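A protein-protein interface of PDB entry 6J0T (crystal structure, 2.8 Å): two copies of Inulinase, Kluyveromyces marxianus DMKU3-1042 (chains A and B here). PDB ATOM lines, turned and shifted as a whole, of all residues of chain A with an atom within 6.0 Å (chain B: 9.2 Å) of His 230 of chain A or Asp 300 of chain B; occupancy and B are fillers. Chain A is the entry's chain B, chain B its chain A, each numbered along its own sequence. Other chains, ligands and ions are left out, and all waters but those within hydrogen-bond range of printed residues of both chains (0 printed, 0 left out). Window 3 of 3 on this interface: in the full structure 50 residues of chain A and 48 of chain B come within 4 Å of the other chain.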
ATOM      1  N   PHE A 208      17.446  13.226  22.466  1.00  0.00           N
ATOM      2  CA  PHE A 208      16.404  13.980  21.772  1.00  0.00           C
ATOM      3  C   PHE A 208      15.021  13.421  22.103  1.00  0.00           C
ATOM      4  O   PHE A 208      14.264  12.992  21.226  1.00  0.00           O
ATOM      5  CB  PHE A 208      16.635  13.971  20.254  1.00  0.00           C
ATOM      6  CG  PHE A 208      18.044  14.259  19.866  1.00  0.00           C
ATOM      7  CD1 PHE A 208      18.533  15.544  19.915  1.00  0.00           C
ATOM      8  CD2 PHE A 208      18.892  13.247  19.488  1.00  0.00           C
ATOM      9  CE1 PHE A 208      19.831  15.806  19.596  1.00  0.00           C
ATOM     10  CE2 PHE A 208      20.185  13.513  19.159  1.00  0.00           C
ATOM     11  CZ  PHE A 208      20.653  14.793  19.215  1.00  0.00           C
ATOM     12  N   PHE A 227       8.448  10.822  23.046  1.00  0.00           N
ATOM     13  CA  PHE A 227       8.472  11.591  21.800  1.00  0.00           C
ATOM     14  C   PHE A 227       9.925  11.872  21.420  1.00  0.00           C
ATOM     15  O   PHE A 227      10.628  12.623  22.119  1.00  0.00           O
ATOM     16  CB  PHE A 227       7.694  12.883  21.999  1.00  0.00           C
ATOM     17  CG  PHE A 227       7.539  13.709  20.766  1.00  0.00           C
ATOM     18  CD1 PHE A 227       6.649  13.349  19.782  1.00  0.00           C
ATOM     19  CD2 PHE A 227       8.244  14.888  20.616  1.00  0.00           C
ATOM     20  CE1 PHE A 227       6.484  14.147  18.664  1.00  0.00           C
ATOM     21  CE2 PHE A 227       8.072  15.683  19.498  1.00  0.00           C
ATOM     22  CZ  PHE A 227       7.198  15.315  18.531  1.00  0.00           C
ATOM     23  N   THR A 228      10.388  11.286  20.317  1.00  0.00           N
ATOM     24  CA  THR A 228      11.827  11.193  20.117  1.00  0.00           C
ATOM     25  C   THR A 228      12.184  11.481  18.662  1.00  0.00           C
ATOM     26  O   THR A 228      11.444  11.125  17.741  1.00  0.00           O
ATOM     27  CB  THR A 228      12.343   9.804  20.617  1.00  0.00           C
ATOM     28  OG1 THR A 228      13.779   9.769  20.637  1.00  0.00           O
ATOM     29  CG2 THR A 228      11.810   8.679  19.770  1.00  0.00           C
ATOM     30  N   HIS A 229      13.293  12.195  18.474  1.00  0.00           N
ATOM     31  CA  HIS A 229      13.895  12.403  17.158  1.00  0.00           C
ATOM     32  C   HIS A 229      12.931  13.074  16.177  1.00  0.00           C
ATOM     33  O   HIS A 229      12.731  12.615  15.046  1.00  0.00           O
ATOM     34  CB  HIS A 229      14.426  11.081  16.599  1.00  0.00           C
ATOM     35  CG  HIS A 229      15.613  10.565  17.346  1.00  0.00           C
ATOM     36  ND1 HIS A 229      15.589  10.331  18.705  1.00  0.00           N
ATOM     37  CD2 HIS A 229      16.872  10.280  16.937  1.00  0.00           C
ATOM     38  CE1 HIS A 229      16.779   9.907  19.099  1.00  0.00           C
ATOM     39  NE2 HIS A 229      17.576   9.869  18.047  1.00  0.00           N
ATOM     40  N   HIS A 230      12.364  14.203  16.605  1.00  0.00           N
ATOM     41  CA  HIS A 230      11.523  15.018  15.746  1.00  0.00           C
ATOM     42  C   HIS A 230      12.171  16.358  15.472  1.00  0.00           C
ATOM     43  O   HIS A 230      13.005  16.831  16.244  1.00  0.00           O
ATOM     44  CB  HIS A 230      10.161  15.286  16.366  1.00  0.00           C
ATOM     45  CG  HIS A 230       9.257  14.107  16.347  1.00  0.00           C
ATOM     46  ND1 HIS A 230       9.420  13.039  17.202  1.00  0.00           N
ATOM     47  CD2 HIS A 230       8.176  13.828  15.586  1.00  0.00           C
ATOM     48  CE1 HIS A 230       8.473  12.150  16.968  1.00  0.00           C
ATOM     49  NE2 HIS A 230       7.705  12.605  15.994  1.00  0.00           N
ATOM     50  N   GLY A 231      11.746  16.958  14.360  1.00  0.00           N
ATOM     51  CA  GLY A 231      12.081  18.335  14.050  1.00  0.00           C
ATOM     52  C   GLY A 231      13.575  18.579  13.891  1.00  0.00           C
ATOM     53  O   GLY A 231      14.282  17.869  13.169  1.00  0.00           O
ATOM     54  N   TRP A 232      14.052  19.622  14.569  1.00  0.00           N
ATOM     55  CA  TRP A 232      15.451  20.030  14.537  1.00  0.00           C
ATOM     56  C   TRP A 232      16.112  19.501  15.799  1.00  0.00           C
ATOM     57  O   TRP A 232      16.037  20.122  16.861  1.00  0.00           O
ATOM     58  CB  TRP A 232      15.571  21.547  14.448  1.00  0.00           C
ATOM     59  CG  TRP A 232      16.968  22.023  14.226  1.00  0.00           C
ATOM     60  CD1 TRP A 232      17.904  22.326  15.179  1.00  0.00           C
ATOM     61  CD2 TRP A 232      17.596  22.243  12.963  1.00  0.00           C
ATOM     62  NE1 TRP A 232      19.078  22.728  14.581  1.00  0.00           N
ATOM     63  CE2 TRP A 232      18.916  22.681  13.221  1.00  0.00           C
ATOM     64  CE3 TRP A 232      17.168  22.120  11.632  1.00  0.00           C
ATOM     65  CZ2 TRP A 232      19.812  22.993  12.196  1.00  0.00           C
ATOM     66  CZ3 TRP A 232      18.063  22.430  10.608  1.00  0.00           C
ATOM     67  CH2 TRP A 232      19.373  22.856  10.901  1.00  0.00           C
ATOM     68  N   THR A 233      16.782  18.363  15.686  1.00  0.00           N
ATOM     69  CA  THR A 233      17.310  17.750  16.897  1.00  0.00           C
ATOM     70  C   THR A 233      18.523  18.501  17.421  1.00  0.00           C
ATOM     71  O   THR A 233      18.707  18.600  18.640  1.00  0.00           O
ATOM     72  CB  THR A 233      17.627  16.282  16.636  1.00  0.00           C
ATOM     73  OG1 THR A 233      18.570  16.182  15.562  1.00  0.00           O
ATOM     74  CG2 THR A 233      16.338  15.545  16.233  1.00  0.00           C
ATOM     75  N   TYR A 237      17.757  18.003  23.146  1.00  0.00           N
ATOM     76  CA  TYR A 237      16.447  18.517  23.522  1.00  0.00           C
ATOM     77  C   TYR A 237      16.531  19.160  24.897  1.00  0.00           C
ATOM     78  O   TYR A 237      17.095  18.572  25.831  1.00  0.00           O
ATOM     79  CB  TYR A 237      15.399  17.409  23.558  1.00  0.00           C
ATOM     80  CG  TYR A 237      14.709  17.159  22.251  1.00  0.00           C
ATOM     81  CD1 TYR A 237      15.319  17.470  21.036  1.00  0.00           C
ATOM     82  CD2 TYR A 237      13.459  16.573  22.217  1.00  0.00           C
ATOM     83  CE1 TYR A 237      14.674  17.214  19.818  1.00  0.00           C
ATOM     84  CE2 TYR A 237      12.816  16.309  21.008  1.00  0.00           C
ATOM     85  CZ  TYR A 237      13.416  16.637  19.817  1.00  0.00           C
ATOM     86  OH  TYR A 237      12.742  16.369  18.636  1.00  0.00           O
ATOM     87  N   GLN A 284      11.858  25.469  18.832  1.00  0.00           N
ATOM     88  CA  GLN A 284      10.912  25.007  17.830  1.00  0.00           C
ATOM     89  C   GLN A 284       9.612  24.540  18.489  1.00  0.00           C
ATOM     90  O   GLN A 284       9.515  24.379  19.711  1.00  0.00           O
ATOM     91  CB  GLN A 284      11.528  23.886  16.987  1.00  0.00           C
ATOM     92  CG  GLN A 284      12.053  22.707  17.794  1.00  0.00           C
ATOM     93  CD  GLN A 284      12.391  21.509  16.920  1.00  0.00           C
ATOM     94  OE1 GLN A 284      11.849  21.337  15.831  1.00  0.00           O
ATOM     95  NE2 GLN A 284      13.289  20.685  17.394  1.00  0.00           N
ATOM     96  N   PHE A 286       5.915  21.935  17.583  1.00  0.00           N
ATOM     97  CA  PHE A 286       5.122  21.050  16.741  1.00  0.00           C
ATOM     98  C   PHE A 286       3.635  21.269  16.986  1.00  0.00           C
ATOM     99  O   PHE A 286       3.227  21.580  18.101  1.00  0.00           O
ATOM    100  CB  PHE A 286       5.484  19.597  17.011  1.00  0.00           C
ATOM    101  CG  PHE A 286       6.959  19.366  17.122  1.00  0.00           C
ATOM    102  CD1 PHE A 286       7.621  19.607  18.318  1.00  0.00           C
ATOM    103  CD2 PHE A 286       7.690  18.929  16.027  1.00  0.00           C
ATOM    104  CE1 PHE A 286       8.984  19.411  18.430  1.00  0.00           C
ATOM    105  CE2 PHE A 286       9.052  18.731  16.131  1.00  0.00           C
ATOM    106  CZ  PHE A 286       9.702  18.966  17.337  1.00  0.00           C
ATOM    107  N   PRO A 297       1.935  14.688  15.960  1.00  0.00           N
ATOM    108  CA  PRO A 297       1.940  15.890  15.133  1.00  0.00           C
ATOM    109  C   PRO A 297       1.145  15.670  13.868  1.00  0.00           C
ATOM    110  O   PRO A 297       0.998  14.541  13.402  1.00  0.00           O
ATOM    111  CB  PRO A 297       3.424  16.096  14.824  1.00  0.00           C
ATOM    112  CG  PRO A 297       4.175  15.216  15.796  1.00  0.00           C
ATOM    113  CD  PRO A 297       3.272  14.079  16.073  1.00  0.00           C
ATOM    114  N   ASP A 299       1.928  16.851  10.941  1.00  0.00           N
ATOM    115  CA  ASP A 299       2.875  16.725   9.837  1.00  0.00           C
ATOM    116  C   ASP A 299       4.253  16.527  10.459  1.00  0.00           C
ATOM    117  O   ASP A 299       4.397  16.491  11.684  1.00  0.00           O
ATOM    118  CB  ASP A 299       2.831  17.939   8.894  1.00  0.00           C
ATOM    119  CG  ASP A 299       2.861  19.289   9.631  1.00  0.00           C
ATOM    120  OD1 ASP A 299       3.548  19.420  10.682  1.00  0.00           O
ATOM    121  OD2 ASP A 299       2.200  20.239   9.140  1.00  0.00           O
ATOM    122  N   ASP A 300       5.272  16.382   9.617  1.00  0.00           N
ATOM    123  CA  ASP A 300       6.643  16.330  10.118  1.00  0.00           C
ATOM    124  C   ASP A 300       7.400  17.624   9.823  1.00  0.00           C
ATOM    125  O   ASP A 300       8.624  17.617   9.651  1.00  0.00           O
ATOM    126  CB  ASP A 300       7.392  15.121   9.560  1.00  0.00           C
ATOM    127  CG  ASP A 300       7.775  15.297   8.104  1.00  0.00           C
ATOM    128  OD1 ASP A 300       7.040  16.029   7.397  1.00  0.00           O
ATOM    129  OD2 ASP A 300       8.797  14.703   7.675  1.00  0.00           O
ATOM    130  N   GLN A 301       6.676  18.736   9.774  1.00  0.00           N
ATOM    131  CA  GLN A 301       7.251  20.040   9.521  1.00  0.00           C
ATOM    132  C   GLN A 301       8.120  20.473  10.693  1.00  0.00           C
ATOM    133  O   GLN A 301       7.960  20.009  11.825  1.00  0.00           O
ATOM    134  CB  GLN A 301       6.140  21.050   9.298  1.00  0.00           C
ATOM    135  CG  GLN A 301       6.492  22.226   8.473  1.00  0.00           C
ATOM    136  CD  GLN A 301       5.309  22.666   7.649  1.00  0.00           C
ATOM    137  OE1 GLN A 301       4.597  21.828   7.099  1.00  0.00           O
ATOM    138  NE2 GLN A 301       5.072  23.982   7.580  1.00  0.00           N
ATOM    139  N   THR A 302       9.054  21.371  10.414  1.00  0.00           N
ATOM    140  CA  THR A 302       9.850  22.008  11.451  1.00  0.00           C
ATOM    141  C   THR A 302       9.480  23.480  11.482  1.00  0.00           C
ATOM    142  O   THR A 302       9.554  24.171  10.462  1.00  0.00           O
ATOM    143  CB  THR A 302      11.339  21.803  11.204  1.00  0.00           C
ATOM    144  OG1 THR A 302      11.668  20.469  11.587  1.00  0.00           O
ATOM    145  CG2 THR A 302      12.168  22.744  12.052  1.00  0.00           C
ATOM    146  N   HIS B 229       4.537  18.836   2.403  1.00  0.00           N
ATOM    147  CA  HIS B 229       4.582  19.517   3.705  1.00  0.00           C
ATOM    148  C   HIS B 229       5.465  18.775   4.707  1.00  0.00           C
ATOM    149  O   HIS B 229       5.056  18.482   5.835  1.00  0.00           O
ATOM    150  CB  HIS B 229       3.176  19.733   4.279  1.00  0.00           C
ATOM    151  CG  HIS B 229       2.393  20.795   3.573  1.00  0.00           C
ATOM    152  ND1 HIS B 229       1.879  20.621   2.305  1.00  0.00           N
ATOM    153  CD2 HIS B 229       2.056  22.054   3.946  1.00  0.00           C
ATOM    154  CE1 HIS B 229       1.255  21.725   1.927  1.00  0.00           C
ATOM    155  NE2 HIS B 229       1.344  22.609   2.907  1.00  0.00           N
ATOM    156  N   HIS B 230       6.703  18.499   4.297  1.00  0.00           N
ATOM    157  CA  HIS B 230       7.686  17.838   5.140  1.00  0.00           C
ATOM    158  C   HIS B 230       8.877  18.746   5.406  1.00  0.00           C
ATOM    159  O   HIS B 230       9.236  19.589   4.580  1.00  0.00           O
ATOM    160  CB  HIS B 230       8.204  16.550   4.505  1.00  0.00           C
ATOM    161  CG  HIS B 230       7.168  15.477   4.360  1.00  0.00           C
ATOM    162  ND1 HIS B 230       7.134  14.360   5.169  1.00  0.00           N
ATOM    163  CD2 HIS B 230       6.165  15.322   3.461  1.00  0.00           C
ATOM    164  CE1 HIS B 230       6.143  13.577   4.787  1.00  0.00           C
ATOM    165  NE2 HIS B 230       5.538  14.138   3.754  1.00  0.00           N
ATOM    166  N   GLY B 231       9.489  18.552   6.568  1.00  0.00           N
ATOM    167  CA  GLY B 231      10.771  19.173   6.850  1.00  0.00           C
ATOM    168  C   GLY B 231      10.676  20.672   7.020  1.00  0.00           C
ATOM    169  O   GLY B 231       9.751  21.198   7.642  1.00  0.00           O
ATOM    170  N   TRP B 232      11.681  21.368   6.497  1.00  0.00           N
ATOM    171  CA  TRP B 232      11.708  22.827   6.448  1.00  0.00           C
ATOM    172  C   TRP B 232      11.097  23.246   5.119  1.00  0.00           C
ATOM    173  O   TRP B 232      11.688  23.012   4.064  1.00  0.00           O
ATOM    174  CB  TRP B 232      13.139  23.349   6.591  1.00  0.00           C
ATOM    175  CG  TRP B 232      13.247  24.834   6.752  1.00  0.00           C
ATOM    176  CD1 TRP B 232      13.242  25.771   5.759  1.00  0.00           C
ATOM    177  CD2 TRP B 232      13.365  25.558   7.982  1.00  0.00           C
ATOM    178  NE1 TRP B 232      13.343  27.032   6.294  1.00  0.00           N
ATOM    179  CE2 TRP B 232      13.420  26.931   7.657  1.00  0.00           C
ATOM    180  CE3 TRP B 232      13.430  25.181   9.329  1.00  0.00           C
ATOM    181  CZ2 TRP B 232      13.550  27.933   8.629  1.00  0.00           C
ATOM    182  CZ3 TRP B 232      13.551  26.187  10.305  1.00  0.00           C
ATOM    183  CH2 TRP B 232      13.607  27.543   9.941  1.00  0.00           C
ATOM    184  N   GLN B 284      17.750  20.688   1.919  1.00  0.00           N
ATOM    185  CA  GLN B 284      17.488  19.708   2.952  1.00  0.00           C
ATOM    186  C   GLN B 284      17.365  18.337   2.310  1.00  0.00           C
ATOM    187  O   GLN B 284      17.216  18.210   1.085  1.00  0.00           O
ATOM    188  CB  GLN B 284      16.206  20.059   3.713  1.00  0.00           C
ATOM    189  CG  GLN B 284      14.949  19.825   2.890  1.00  0.00           C
ATOM    190  CD  GLN B 284      13.667  20.116   3.654  1.00  0.00           C
ATOM    191  OE1 GLN B 284      13.567  19.874   4.861  1.00  0.00           O
ATOM    192  NE2 GLN B 284      12.674  20.639   2.942  1.00  0.00           N
ATOM    193  N   TYR B 285      17.408  17.300   3.152  1.00  0.00           N
ATOM    194  CA  TYR B 285      17.198  15.935   2.688  1.00  0.00           C
ATOM    195  C   TYR B 285      16.419  15.131   3.727  1.00  0.00           C
ATOM    196  O   TYR B 285      16.434  15.429   4.927  1.00  0.00           O
ATOM    197  CB  TYR B 285      18.530  15.219   2.356  1.00  0.00           C
ATOM    198  CG  TYR B 285      19.499  15.033   3.526  1.00  0.00           C
ATOM    199  CD1 TYR B 285      20.477  15.990   3.816  1.00  0.00           C
ATOM    200  CD2 TYR B 285      19.464  13.891   4.300  1.00  0.00           C
ATOM    201  CE1 TYR B 285      21.350  15.826   4.858  1.00  0.00           C
ATOM    202  CE2 TYR B 285      20.346  13.712   5.352  1.00  0.00           C
ATOM    203  CZ  TYR B 285      21.279  14.682   5.628  1.00  0.00           C
ATOM    204  OH  TYR B 285      22.145  14.494   6.683  1.00  0.00           O
ATOM    205  N   PHE B 286      15.761  14.077   3.233  1.00  0.00           N
ATOM    206  CA  PHE B 286      15.041  13.097   4.035  1.00  0.00           C
ATOM    207  C   PHE B 286      15.603  11.696   3.806  1.00  0.00           C
ATOM    208  O   PHE B 286      15.971  11.348   2.680  1.00  0.00           O
ATOM    209  CB  PHE B 286      13.542  13.134   3.694  1.00  0.00           C
ATOM    210  CG  PHE B 286      12.938  14.499   3.844  1.00  0.00           C
ATOM    211  CD1 PHE B 286      12.453  14.922   5.069  1.00  0.00           C
ATOM    212  CD2 PHE B 286      12.895  15.377   2.772  1.00  0.00           C
ATOM    213  CE1 PHE B 286      11.911  16.189   5.218  1.00  0.00           C
ATOM    214  CE2 PHE B 286      12.360  16.636   2.912  1.00  0.00           C
ATOM    215  CZ  PHE B 286      11.868  17.047   4.145  1.00  0.00           C
ATOM    216  N   VAL B 287      15.641  10.897   4.877  1.00  0.00           N
ATOM    217  CA  VAL B 287      16.093   9.505   4.868  1.00  0.00           C
ATOM    218  C   VAL B 287      14.875   8.590   4.994  1.00  0.00           C
ATOM    219  O   VAL B 287      14.070   8.751   5.918  1.00  0.00           O
ATOM    220  CB  VAL B 287      17.070   9.237   6.028  1.00  0.00           C
ATOM    221  CG1 VAL B 287      17.680   7.869   5.904  1.00  0.00           C
ATOM    222  CG2 VAL B 287      18.128  10.336   6.127  1.00  0.00           C
ATOM    223  N   THR B 296       8.603   7.194   1.989  1.00  0.00           N
ATOM    224  CA  THR B 296       8.228   7.156   3.398  1.00  0.00           C
ATOM    225  C   THR B 296       9.458   7.441   4.231  1.00  0.00           C
ATOM    226  O   THR B 296      10.391   6.614   4.257  1.00  0.00           O
ATOM    227  CB  THR B 296       7.641   5.802   3.796  1.00  0.00           C
ATOM    228  OG1 THR B 296       6.496   5.498   2.983  1.00  0.00           O
ATOM    229  CG2 THR B 296       7.250   5.833   5.273  1.00  0.00           C
ATOM    230  N   PRO B 297       9.507   8.582   4.902  1.00  0.00           N
ATOM    231  CA  PRO B 297      10.692   8.921   5.698  1.00  0.00           C
ATOM    232  C   PRO B 297      10.772   8.090   6.970  1.00  0.00           C
ATOM    233  O   PRO B 297       9.779   7.921   7.678  1.00  0.00           O
ATOM    234  CB  PRO B 297      10.478  10.406   6.020  1.00  0.00           C
ATOM    235  CG  PRO B 297       9.456  10.902   5.012  1.00  0.00           C
ATOM    236  CD  PRO B 297       8.596   9.723   4.705  1.00  0.00           C
ATOM    237  N   ILE B 298      11.981   7.606   7.280  1.00  0.00           N
ATOM    238  CA  ILE B 298      12.185   6.837   8.513  1.00  0.00           C
ATOM    239  C   ILE B 298      11.685   7.603   9.727  1.00  0.00           C
ATOM    240  O   ILE B 298      11.110   7.016  10.648  1.00  0.00           O
ATOM    241  CB  ILE B 298      13.667   6.447   8.695  1.00  0.00           C
ATOM    242  CG1 ILE B 298      14.508   7.662   9.098  1.00  0.00           C
ATOM    243  CG2 ILE B 298      14.212   5.766   7.465  1.00  0.00           C
ATOM    244  CD1 ILE B 298      16.003   7.428   9.094  1.00  0.00           C
ATOM    245  N   ASP B 299      11.896   8.921   9.754  1.00  0.00           N
ATOM    246  CA  ASP B 299      11.660   9.723  10.946  1.00  0.00           C
ATOM    247  C   ASP B 299      11.075  11.066  10.537  1.00  0.00           C
ATOM    248  O   ASP B 299      10.747  11.301   9.371  1.00  0.00           O
ATOM    249  CB  ASP B 299      12.942   9.863  11.781  1.00  0.00           C
ATOM    250  CG  ASP B 299      14.085  10.574  11.045  1.00  0.00           C
ATOM    251  OD1 ASP B 299      13.860  11.334  10.061  1.00  0.00           O
ATOM    252  OD2 ASP B 299      15.238  10.344  11.484  1.00  0.00           O
ATOM    253  N   ASP B 300      10.921  11.951  11.512  1.00  0.00           N
ATOM    254  CA  ASP B 300      10.328  13.259  11.276  1.00  0.00           C
ATOM    255  C   ASP B 300      11.356  14.371  11.472  1.00  0.00           C
ATOM    256  O   ASP B 300      11.006  15.512  11.797  1.00  0.00           O
ATOM    257  CB  ASP B 300       9.115  13.443  12.185  1.00  0.00           C
ATOM    258  CG  ASP B 300       8.304  12.143  12.356  1.00  0.00           C
ATOM    259  OD1 ASP B 300       8.783  11.258  13.125  1.00  0.00           O
ATOM    260  OD2 ASP B 300       7.224  11.991  11.711  1.00  0.00           O
ATOM    261  N   GLN B 301      12.630  14.046  11.269  1.00  0.00           N
ATOM    262  CA  GLN B 301      13.728  14.976  11.485  1.00  0.00           C
ATOM    263  C   GLN B 301      13.924  15.884  10.269  1.00  0.00           C
ATOM    264  O   GLN B 301      13.531  15.552   9.147  1.00  0.00           O
ATOM    265  CB  GLN B 301      15.010  14.195  11.771  1.00  0.00           C
ATOM    266  CG  GLN B 301      15.837  14.746  12.890  1.00  0.00           C
ATOM    267  CD  GLN B 301      16.954  13.799  13.306  1.00  0.00           C
ATOM    268  OE1 GLN B 301      18.118  14.198  13.418  1.00  0.00           O
ATOM    269  NE2 GLN B 301      16.601  12.542  13.550  1.00  0.00           N
ATOM    270  N   THR B 302      14.512  17.052  10.510  1.00  0.00           N
ATOM    271  CA  THR B 302      14.913  17.973   9.454  1.00  0.00           C
ATOM    272  C   THR B 302      16.429  17.975   9.347  1.00  0.00           C
ATOM    273  O   THR B 302      17.128  18.158  10.347  1.00  0.00           O
ATOM    274  CB  THR B 302      14.386  19.389   9.708  1.00  0.00           C
ATOM    275  OG1 THR B 302      12.984  19.400   9.439  1.00  0.00           O
ATOM    276  CG2 THR B 302      15.015  20.379   8.762  1.00  0.00           C
ATOM    277  N   ARG B 303      16.934  17.760   8.140  1.00  0.00           N
ATOM    278  CA  ARG B 303      18.361  17.583   7.923  1.00  0.00           C
ATOM    279  C   ARG B 303      18.802  18.471   6.781  1.00  0.00           C
ATOM    280  O   ARG B 303      18.266  18.380   5.675  1.00  0.00           O
ATOM    281  CB  ARG B 303      18.691  16.133   7.597  1.00  0.00           C
ATOM    282  CG  ARG B 303      18.690  15.253   8.776  1.00  0.00           C
ATOM    283  CD  ARG B 303      18.637  13.840   8.307  1.00  0.00           C
ATOM    284  NE  ARG B 303      18.770  12.932   9.427  1.00  0.00           N
ATOM    285  CZ  ARG B 303      17.783  12.170   9.854  1.00  0.00           C
ATOM    286  NH1 ARG B 303      17.976  11.368  10.882  1.00  0.00           N
ATOM    287  NH2 ARG B 303      16.611  12.216   9.238  1.00  0.00           N
ATOM    288  N   ASP B 369      21.825   8.211  15.809  1.00  0.00           N
ATOM    289  CA  ASP B 369      21.081   8.791  14.701  1.00  0.00           C
ATOM    290  C   ASP B 369      21.775   8.377  13.403  1.00  0.00           C
ATOM    291  O   ASP B 369      22.609   7.465  13.372  1.00  0.00           O
ATOM    292  CB  ASP B 369      20.972  10.313  14.882  1.00  0.00           C
ATOM    293  CG  ASP B 369      19.718  10.884  14.249  1.00  0.00           C
ATOM    294  OD1 ASP B 369      19.238  10.290  13.254  1.00  0.00           O
ATOM    295  OD2 ASP B 369      19.210  11.915  14.755  1.00  0.00           O
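A ring nitrogen (ND1) of His 230 of chain B lies within hydrogen-bond range of the side-chain carboxylate (OD1) of Asp 300 of chain A, 2.8 Å away.
The side-chain hydroxyl (OG1) of Thr 302 of chain B is in hydrogen-bond range of the side-chain hydroxyl (OG1) of Thr 302 of chain A, 2.7 Å away.
The backbone NH (N) of Gly 231 of chain B is in hydrogen-bond range of the backbone carbonyl oxygen (O) of Asp 300 of chain A, 3.3 Å away.
The backbone carbonyl oxygen (O) of Asp 300 of chain B is in hydrogen-bond range of the backbone NH (N) of Gly 231 of chain A (3.0 Å).
The backbone NH (N) of Thr 302 of chain B lies within hydrogen-bond range of the backbone carbonyl oxygen (O) of Gly 231 of chain A (2.8 Å).
The side-chain amide oxygen (OE1) of Gln 301 of chain B lies within hydrogen-bond range of the side-chain hydroxyl (OG1) of Thr 233 of chain A (3.0 Å).
A ring nitrogen (NE2) of His 230 of chain A is in hydrogen-bond range of the side-chain carboxylate (OD1) of Asp 300 of chain B (3.3 Å).
O of Gly 231 of chain B sits at hydrogen-bond distance from N of Thr 302 of chain A.
The side-chain amide nitrogen (NE2) of Gln 284 of chain B sits at hydrogen-bond distance from the backbone carbonyl oxygen (O) of Trp 232 of chain B (2.8 Å).
The backbone NH (N) of Gln 301 of chain A lies within hydrogen-bond range of the side-chain carboxylate (OD1) of Asp 299 of chain A.
A ring nitrogen (ND1) of His 230 of chain A sits at hydrogen-bond distance from the backbone carbonyl oxygen (O) of Thr 228 of chain A, at 2.8 Å.
NH1 of Arg 303 of chain B is in salt-bridge range of OD1 of Asp 369 of chain B (2.9 Å).
O of Trp 232 of chain A lies within hydrogen-bond range of NE2 of Gln 284 of chain A (2.9 Å).
Among the printed residues, merely in contact across the chains: His 229 of chain A with Asp 369 of chain B (3.6 Å), Gly 231 of chain A with Gln 301 of chain B (3.4 Å), Trp 232 of chain A with Thr 302 of chain B (3.99 Å), Asp 299 of chain A with His 229 of chain B (3.8 Å), Asp 300 of chain A with His 229 of chain B (3.5 Å), Asp 300 of chain A with Asp 300 of chain B (3.6 Å), Gln 301 of chain A with His 229 of chain B (3.6 Å), Gln 301 of chain A with Gly 231 of chain B (3.3 Å) and Thr 302 of chain A with Trp 232 of chain B (3.9 Å).
His 230 of chain A touches just one residue of chain B: Asp 300 (3.3 Å).
Of chain A, only His 230, Gly 231 and Asp 300 come within 4 Å of Asp 300 of chain B.
Of the printed residues of chain A, Asp 369 of chain B touches His 229 (3.6 Å).
Printed residues of chain B within 4 Å of Thr 233 of chain A: Gln 301.
Of the printed residues of chain B, Trp 232 of chain A touches Thr 302 (3.99 Å).
Printed residues of chain A within 4 Å of His 230 of chain B: Asp 300.
Phe 286 of chain A touches none of the printed residues of chain B.
The nearest residue of chain A that does not touch Asp 300 of chain B is His 229 of chain A (4.03 Å).
The nearest printed residue of chain A that does not touch Gln 301 of chain B is His 229 of chain A (4.02 Å).
Of the 16 printed residues of chain A, 9 touch a printed residue of chain B.
Hydrophobic or aromatic side chains of chain B that line the printed part of chain A: His 229, His 230 and Trp 232.
Along chain B the printed residues that touch a printed residue of chain A span positions 229 to 369.
Among the printed residues, no Asp or Glu carboxylate lies within 4 Å of a Lys or Arg side-chain nitrogen of the other chain.
Gly 231 of chain A touches Asp 300 of chain B, and with the chains exchanged Asp 300 of chain A touches Gly 231 of chain B.
Gly 231 of chain A touches Gln 301 of chain B, and with the chains exchanged Gln 301 of chain A touches Gly 231 of chain B.
Asp 300 of chain A touches His 229 of chain B, but with the chains exchanged His 229 of chain A does not touch Asp 300 of chain B (4.03 Å).
Asp 300 of chain B touches its own counterpart, Asp 300 of chain A.
Of the 17 pairs that touch across the chains among the printed residues, 12 have their exchanged pair printed and touching as well.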
